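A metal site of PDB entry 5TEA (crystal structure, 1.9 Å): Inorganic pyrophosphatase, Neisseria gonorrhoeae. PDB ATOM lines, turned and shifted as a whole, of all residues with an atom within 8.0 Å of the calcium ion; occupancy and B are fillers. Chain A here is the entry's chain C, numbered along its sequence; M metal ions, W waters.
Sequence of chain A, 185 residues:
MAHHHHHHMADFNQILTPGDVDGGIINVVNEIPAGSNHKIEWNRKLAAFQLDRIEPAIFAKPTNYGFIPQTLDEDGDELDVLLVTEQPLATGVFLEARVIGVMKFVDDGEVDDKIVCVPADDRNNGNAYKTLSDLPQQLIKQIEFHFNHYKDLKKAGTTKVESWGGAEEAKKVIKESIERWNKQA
N of Asp 112 is in hydrogen-bond range of O of Phe 105 (2.9 Å).
O of Asp 112 lies within hydrogen-bond range of NZ of Lys 114 (3.1 Å).
The side-chain amino group (NZ) of Lys 114 sits close to the side-chain carboxylate (OD2) of Asp 80, at 2.9 Å.
OD1 of Asp 75 sits at hydrogen-bond distance from N of Asp 77 (2.9 Å).
The side-chain carboxylate (OD2) of Asp 80 sits close to the side-chain hydroxyl (OH) of Tyr 65, at 3.0 Å.
Along chain A the residues within 4 Å of the calcium ion span positions 75 to 112.
OD2 of Asp 75 binds the calcium ion (2.3 Å).
Water W3 is bound to the calcium ion (2.3 Å).
OD2 of Asp 80 is bound to the calcium ion (2.3 Å).
Water W1 binds the calcium ion (2.4 Å).
The calcium ion is bound by OD1 of Asp 112 (2.4 Å).
The side-chain carboxylate (OD1) of Asp 80 is bound to the calcium ion (2.8 Å).
OD2 of Asp 112 binds the calcium ion, at 2.8 Å.
The calcium ion is bound by water W2, 2.9 Å away.
The calcium ion has eight donor atoms within binding distance.
Water W3 bridges O of Glu 78 (2.8 Å) and OD1 of Asp 75 (2.8 Å).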
ATOM      1  N   GLU A  31       1.989  11.940  21.933  1.00  0.00           N
ATOM      2  CA  GLU A  31       3.165  11.709  22.775  1.00  0.00           C
ATOM      3  C   GLU A  31       4.447  12.267  22.178  1.00  0.00           C
ATOM      4  O   GLU A  31       5.233  12.898  22.888  1.00  0.00           O
ATOM      5  CB  GLU A  31       3.349  10.208  23.036  1.00  0.00           C
ATOM      6  CG  GLU A  31       2.301   9.599  23.933  1.00  0.00           C
ATOM      7  CD  GLU A  31       2.280   8.086  23.826  1.00  0.00           C
ATOM      8  OE1 GLU A  31       2.015   7.566  22.707  1.00  0.00           O
ATOM      9  OE2 GLU A  31       2.528   7.414  24.844  1.00  0.00           O
ATOM     10  N   LYS A  39      12.003   9.440  22.617  1.00  0.00           N
ATOM     11  CA  LYS A  39      10.939   8.470  22.836  1.00  0.00           C
ATOM     12  C   LYS A  39      10.195   8.887  24.100  1.00  0.00           C
ATOM     13  O   LYS A  39      10.658   8.668  25.221  1.00  0.00           O
ATOM     14  CB  LYS A  39      11.476   7.038  22.933  1.00  0.00           C
ATOM     15  CG  LYS A  39      10.355   5.997  23.043  1.00  0.00           C
ATOM     16  CD  LYS A  39      10.896   4.574  23.287  1.00  0.00           C
ATOM     17  CE  LYS A  39       9.769   3.540  23.282  1.00  0.00           C
ATOM     18  NZ  LYS A  39       8.795   3.716  24.396  1.00  0.00           N
ATOM     19  N   GLU A  41       6.579   8.746  26.292  1.00  0.00           N
ATOM     20  CA  GLU A  41       5.452   7.854  26.510  1.00  0.00           C
ATOM     21  C   GLU A  41       4.620   8.399  27.658  1.00  0.00           C
ATOM     22  O   GLU A  41       5.173   8.876  28.645  1.00  0.00           O
ATOM     23  CB  GLU A  41       5.967   6.448  26.787  1.00  0.00           C
ATOM     24  CG  GLU A  41       5.000   5.480  27.384  1.00  0.00           C
ATOM     25  CD  GLU A  41       5.698   4.183  27.770  1.00  0.00           C
ATOM     26  OE1 GLU A  41       6.735   4.263  28.460  1.00  0.00           O
ATOM     27  OE2 GLU A  41       5.228   3.105  27.352  1.00  0.00           O
ATOM     28  N   TYR A  65       3.354  10.542  17.063  1.00  0.00           N
ATOM     29  CA  TYR A  65       3.119   9.264  17.702  1.00  0.00           C
ATOM     30  C   TYR A  65       2.244   9.499  18.926  1.00  0.00           C
ATOM     31  O   TYR A  65       2.598  10.303  19.786  1.00  0.00           O
ATOM     32  CB  TYR A  65       4.445   8.624  18.085  1.00  0.00           C
ATOM     33  CG  TYR A  65       4.397   7.138  18.324  1.00  0.00           C
ATOM     34  CD1 TYR A  65       4.600   6.243  17.282  1.00  0.00           C
ATOM     35  CD2 TYR A  65       4.192   6.633  19.593  1.00  0.00           C
ATOM     36  CE1 TYR A  65       4.594   4.849  17.522  1.00  0.00           C
ATOM     37  CE2 TYR A  65       4.170   5.268  19.833  1.00  0.00           C
ATOM     38  CZ  TYR A  65       4.368   4.380  18.787  1.00  0.00           C
ATOM     39  OH  TYR A  65       4.354   3.042  19.041  1.00  0.00           O
ATOM     40  N   GLY A  66       1.118   8.795  19.016  1.00  0.00           N
ATOM     41  CA  GLY A  66       0.195   8.995  20.116  1.00  0.00           C
ATOM     42  C   GLY A  66      -0.506   7.734  20.580  1.00  0.00           C
ATOM     43  O   GLY A  66      -0.061   6.633  20.214  1.00  0.00           O
ATOM     44  N   PHE A  67      -1.581   7.851  21.380  1.00  0.00           N
ATOM     45  CA  PHE A  67      -2.348   6.684  21.826  1.00  0.00           C
ATOM     46  C   PHE A  67      -3.827   7.043  21.936  1.00  0.00           C
ATOM     47  O   PHE A  67      -4.227   8.211  21.961  1.00  0.00           O
ATOM     48  CB  PHE A  67      -1.828   6.144  23.169  1.00  0.00           C
ATOM     49  CG  PHE A  67      -2.080   7.043  24.339  1.00  0.00           C
ATOM     50  CD1 PHE A  67      -1.201   8.084  24.643  1.00  0.00           C
ATOM     51  CD2 PHE A  67      -3.192   6.866  25.145  1.00  0.00           C
ATOM     52  CE1 PHE A  67      -1.430   8.915  25.737  1.00  0.00           C
ATOM     53  CE2 PHE A  67      -3.429   7.696  26.245  1.00  0.00           C
ATOM     54  CZ  PHE A  67      -2.551   8.725  26.531  1.00  0.00           C
ATOM     55  N   ASP A  73      -3.495  -2.614  24.147  1.00  0.00           N
ATOM     56  CA  ASP A  73      -2.980  -3.573  23.184  1.00  0.00           C
ATOM     57  C   ASP A  73      -2.213  -4.630  23.981  1.00  0.00           C
ATOM     58  O   ASP A  73      -2.278  -4.670  25.204  1.00  0.00           O
ATOM     59  CB  ASP A  73      -2.147  -2.858  22.112  1.00  0.00           C
ATOM     60  CG  ASP A  73      -2.061  -3.649  20.808  1.00  0.00           C
ATOM     61  OD1 ASP A  73      -2.502  -4.821  20.785  1.00  0.00           O
ATOM     62  OD2 ASP A  73      -1.559  -3.097  19.804  1.00  0.00           O
ATOM     63  N   GLU A  74      -1.484  -5.499  23.285  1.00  0.00           N
ATOM     64  CA  GLU A  74      -0.872  -6.631  23.981  1.00  0.00           C
ATOM     65  C   GLU A  74       0.334  -6.213  24.829  1.00  0.00           C
ATOM     66  O   GLU A  74       0.606  -6.857  25.848  1.00  0.00           O
ATOM     67  CB  GLU A  74      -0.498  -7.714  22.975  1.00  0.00           C
ATOM     68  CG  GLU A  74      -1.726  -8.350  22.318  1.00  0.00           C
ATOM     69  CD  GLU A  74      -1.409  -9.553  21.459  1.00  0.00           C
ATOM     70  OE1 GLU A  74      -0.263 -10.067  21.525  1.00  0.00           O
ATOM     71  OE2 GLU A  74      -2.312  -9.993  20.703  1.00  0.00           O
ATOM     72  N   ASP A  75       1.040  -5.121  24.454  1.00  0.00           N
ATOM     73  CA  ASP A  75       2.201  -4.644  25.226  1.00  0.00           C
ATOM     74  C   ASP A  75       1.802  -4.044  26.598  1.00  0.00           C
ATOM     75  O   ASP A  75       2.676  -3.544  27.330  1.00  0.00           O
ATOM     76  CB  ASP A  75       3.038  -3.643  24.418  1.00  0.00           C
ATOM     77  CG  ASP A  75       2.324  -2.304  24.144  1.00  0.00           C
ATOM     78  OD1 ASP A  75       1.150  -2.114  24.542  1.00  0.00           O
ATOM     79  OD2 ASP A  75       2.974  -1.412  23.503  1.00  0.00           O
ATOM     80  N   GLY A  76       0.509  -4.097  26.929  1.00  0.00           N
ATOM     81  CA  GLY A  76       0.019  -3.569  28.184  1.00  0.00           C
ATOM     82  C   GLY A  76      -0.169  -2.068  28.197  1.00  0.00           C
ATOM     83  O   GLY A  76      -0.585  -1.531  29.230  1.00  0.00           O
ATOM     84  N   ASP A  77       0.133  -1.379  27.101  1.00  0.00           N
ATOM     85  CA  ASP A  77      -0.066   0.056  26.967  1.00  0.00           C
ATOM     86  C   ASP A  77      -1.298   0.309  26.110  1.00  0.00           C
ATOM     87  O   ASP A  77      -1.834  -0.598  25.469  1.00  0.00           O
ATOM     88  CB  ASP A  77       1.160   0.732  26.338  1.00  0.00           C
ATOM     89  CG  ASP A  77       2.415   0.562  27.157  1.00  0.00           C
ATOM     90  OD1 ASP A  77       2.321   0.462  28.398  1.00  0.00           O
ATOM     91  OD2 ASP A  77       3.504   0.549  26.544  1.00  0.00           O
ATOM     92  N   GLU A  78      -1.733   1.575  26.093  1.00  0.00           N
ATOM     93  CA  GLU A  78      -2.822   1.961  25.221  1.00  0.00           C
ATOM     94  C   GLU A  78      -2.423   1.743  23.764  1.00  0.00           C
ATOM     95  O   GLU A  78      -1.238   1.741  23.407  1.00  0.00           O
ATOM     96  CB  GLU A  78      -3.223   3.424  25.443  1.00  0.00           C
ATOM     97  CG  GLU A  78      -3.759   3.745  26.863  1.00  0.00           C
ATOM     98  CD  GLU A  78      -2.650   4.054  27.875  1.00  0.00           C
ATOM     99  OE1 GLU A  78      -1.472   3.739  27.618  1.00  0.00           O
ATOM    100  OE2 GLU A  78      -2.966   4.631  28.938  1.00  0.00           O
ATOM    101  N   LEU A  79      -3.430   1.555  22.922  1.00  0.00           N
ATOM    102  CA  LEU A  79      -3.191   1.302  21.504  1.00  0.00           C
ATOM    103  C   LEU A  79      -2.526   2.509  20.850  1.00  0.00           C
ATOM    104  O   LEU A  79      -2.957   3.652  21.068  1.00  0.00           O
ATOM    105  CB  LEU A  79      -4.531   0.973  20.839  1.00  0.00           C
ATOM    106  CG  LEU A  79      -4.606   0.785  19.325  1.00  0.00           C
ATOM    107  CD1 LEU A  79      -3.640  -0.278  18.880  1.00  0.00           C
ATOM    108  CD2 LEU A  79      -6.059   0.431  18.894  1.00  0.00           C
ATOM    109  N   ASP A  80      -1.457   2.280  20.089  1.00  0.00           N
ATOM    110  CA  ASP A  80      -0.662   3.370  19.525  1.00  0.00           C
ATOM    111  C   ASP A  80      -1.350   4.013  18.310  1.00  0.00           C
ATOM    112  O   ASP A  80      -2.144   3.381  17.607  1.00  0.00           O
ATOM    113  CB  ASP A  80       0.714   2.886  19.058  1.00  0.00           C
ATOM    114  CG  ASP A  80       1.489   2.177  20.133  1.00  0.00           C
ATOM    115  OD1 ASP A  80       1.485   2.638  21.298  1.00  0.00           O
ATOM    116  OD2 ASP A  80       2.103   1.139  19.788  1.00  0.00           O
ATOM    117  N   VAL A  81      -0.967   5.260  18.027  1.00  0.00           N
ATOM    118  CA  VAL A  81      -1.507   6.015  16.895  1.00  0.00           C
ATOM    119  C   VAL A  81      -0.353   6.644  16.126  1.00  0.00           C
ATOM    120  O   VAL A  81       0.555   7.247  16.727  1.00  0.00           O
ATOM    121  CB  VAL A  81      -2.485   7.113  17.346  1.00  0.00           C
ATOM    122  CG1 VAL A  81      -2.911   7.992  16.149  1.00  0.00           C
ATOM    123  CG2 VAL A  81      -3.718   6.490  18.006  1.00  0.00           C
ATOM    124  N   PHE A 105       1.732  -4.828  13.148  1.00  0.00           N
ATOM    125  CA  PHE A 105       3.119  -4.679  13.564  1.00  0.00           C
ATOM    126  C   PHE A 105       3.449  -5.635  14.684  1.00  0.00           C
ATOM    127  O   PHE A 105       2.634  -5.849  15.586  1.00  0.00           O
ATOM    128  CB  PHE A 105       3.372  -3.228  13.998  1.00  0.00           C
ATOM    129  CG  PHE A 105       4.816  -2.902  14.320  1.00  0.00           C
ATOM    130  CD1 PHE A 105       5.813  -3.072  13.374  1.00  0.00           C
ATOM    131  CD2 PHE A 105       5.157  -2.383  15.560  1.00  0.00           C
ATOM    132  CE1 PHE A 105       7.137  -2.766  13.676  1.00  0.00           C
ATOM    133  CE2 PHE A 105       6.468  -2.042  15.867  1.00  0.00           C
ATOM    134  CZ  PHE A 105       7.463  -2.249  14.928  1.00  0.00           C
ATOM    135  N   ASP A 107       6.606  -6.224  17.422  1.00  0.00           N
ATOM    136  CA  ASP A 107       7.783  -5.600  18.001  1.00  0.00           C
ATOM    137  C   ASP A 107       8.308  -6.552  19.056  1.00  0.00           C
ATOM    138  O   ASP A 107       7.643  -6.765  20.073  1.00  0.00           O
ATOM    139  CB  ASP A 107       7.397  -4.236  18.600  1.00  0.00           C
ATOM    140  CG  ASP A 107       8.588  -3.342  18.862  1.00  0.00           C
ATOM    141  OD1 ASP A 107       9.674  -3.860  19.166  1.00  0.00           O
ATOM    142  OD2 ASP A 107       8.426  -2.092  18.776  1.00  0.00           O
ATOM    143  N   GLU A 110       5.847  -9.355  20.232  1.00  0.00           N
ATOM    144  CA  GLU A 110       4.455  -9.095  20.554  1.00  0.00           C
ATOM    145  C   GLU A 110       3.791  -8.198  19.528  1.00  0.00           C
ATOM    146  O   GLU A 110       4.434  -7.364  18.886  1.00  0.00           O
ATOM    147  CB  GLU A 110       4.288  -8.495  21.952  1.00  0.00           C
ATOM    148  CG  GLU A 110       5.107  -7.259  22.228  1.00  0.00           C
ATOM    149  CD  GLU A 110       4.982  -6.837  23.681  1.00  0.00           C
ATOM    150  OE1 GLU A 110       4.315  -7.560  24.450  1.00  0.00           O
ATOM    151  OE2 GLU A 110       5.559  -5.787  24.049  1.00  0.00           O
ATOM    152  N   VAL A 111       2.483  -8.389  19.386  1.00  0.00           N
ATOM    153  CA  VAL A 111       1.694  -7.530  18.519  1.00  0.00           C
ATOM    154  C   VAL A 111       1.642  -6.130  19.098  1.00  0.00           C
ATOM    155  O   VAL A 111       1.385  -5.934  20.299  1.00  0.00           O
ATOM    156  CB  VAL A 111       0.286  -8.116  18.341  1.00  0.00           C
ATOM    157  CG1 VAL A 111      -0.569  -7.160  17.487  1.00  0.00           C
ATOM    158  CG2 VAL A 111       0.379  -9.503  17.720  1.00  0.00           C
ATOM    159  N   ASP A 112       1.895  -5.133  18.268  1.00  0.00           N
ATOM    160  CA  ASP A 112       1.878  -3.754  18.683  1.00  0.00           C
ATOM    161  C   ASP A 112       1.385  -2.941  17.490  1.00  0.00           C
ATOM    162  O   ASP A 112       2.097  -2.123  16.927  1.00  0.00           O
ATOM    163  CB  ASP A 112       3.260  -3.322  19.165  1.00  0.00           C
ATOM    164  CG  ASP A 112       3.208  -2.065  20.017  1.00  0.00           C
ATOM    165  OD1 ASP A 112       2.152  -1.793  20.613  1.00  0.00           O
ATOM    166  OD2 ASP A 112       4.243  -1.356  20.100  1.00  0.00           O
ATOM    167  N   ASP A 113       0.129  -3.183  17.091  1.00  0.00           N
ATOM    168  CA  ASP A 113      -0.475  -2.499  15.950  1.00  0.00           C
ATOM    169  C   ASP A 113      -0.595  -0.995  16.215  1.00  0.00           C
ATOM    170  O   ASP A 113      -0.647  -0.539  17.355  1.00  0.00           O
ATOM    171  CB  ASP A 113      -1.867  -3.075  15.637  1.00  0.00           C
ATOM    172  CG  ASP A 113      -1.839  -4.566  15.312  1.00  0.00           C
ATOM    173  OD1 ASP A 113      -0.820  -5.063  14.795  1.00  0.00           O
ATOM    174  OD2 ASP A 113      -2.871  -5.245  15.549  1.00  0.00           O
ATOM    175  N   LYS A 114      -0.646  -0.226  15.133  1.00  0.00           N
ATOM    176  CA  LYS A 114      -0.690   1.229  15.232  1.00  0.00           C
ATOM    177  C   LYS A 114      -1.760   1.759  14.296  1.00  0.00           C
ATOM    178  O   LYS A 114      -1.750   1.467  13.100  1.00  0.00           O
ATOM    179  CB  LYS A 114       0.685   1.818  14.905  1.00  0.00           C
ATOM    180  CG  LYS A 114       1.788   1.148  15.720  1.00  0.00           C
ATOM    181  CD  LYS A 114       3.031   1.993  15.866  1.00  0.00           C
ATOM    182  CE  LYS A 114       4.187   1.130  16.358  1.00  0.00           C
ATOM    183  NZ  LYS A 114       3.814   0.329  17.541  1.00  0.00           N
ATOM    184  N   TYR A 150      13.965   0.616  13.030  1.00  0.00           N
ATOM    185  CA  TYR A 150      14.357   1.633  14.015  1.00  0.00           C
ATOM    186  C   TYR A 150      15.108   1.064  15.221  1.00  0.00           C
ATOM    187  O   TYR A 150      15.682   1.842  15.982  1.00  0.00           O
ATOM    188  CB  TYR A 150      13.142   2.440  14.485  1.00  0.00           C
ATOM    189  CG  TYR A 150      12.238   1.787  15.514  1.00  0.00           C
ATOM    190  CD1 TYR A 150      11.406   0.721  15.184  1.00  0.00           C
ATOM    191  CD2 TYR A 150      12.183   2.280  16.811  1.00  0.00           C
ATOM    192  CE1 TYR A 150      10.563   0.145  16.124  1.00  0.00           C
ATOM    193  CE2 TYR A 150      11.353   1.709  17.767  1.00  0.00           C
ATOM    194  CZ  TYR A 150      10.544   0.645  17.419  1.00  0.00           C
ATOM    195  OH  TYR A 150       9.717   0.083  18.365  1.00  0.00           O
HETATM  196 CA    CA M   1       2.723   0.233  21.864  1.00  0.00          CA
HETATM  197  O   HOH W   1       2.954   1.637  23.849  1.00  0.00           O
HETATM  198  O   HOH W   2       4.880   2.111  21.514  1.00  0.00           O
HETATM  199  O   HOH W   3       0.535  -0.230  22.570  1.00  0.00           O
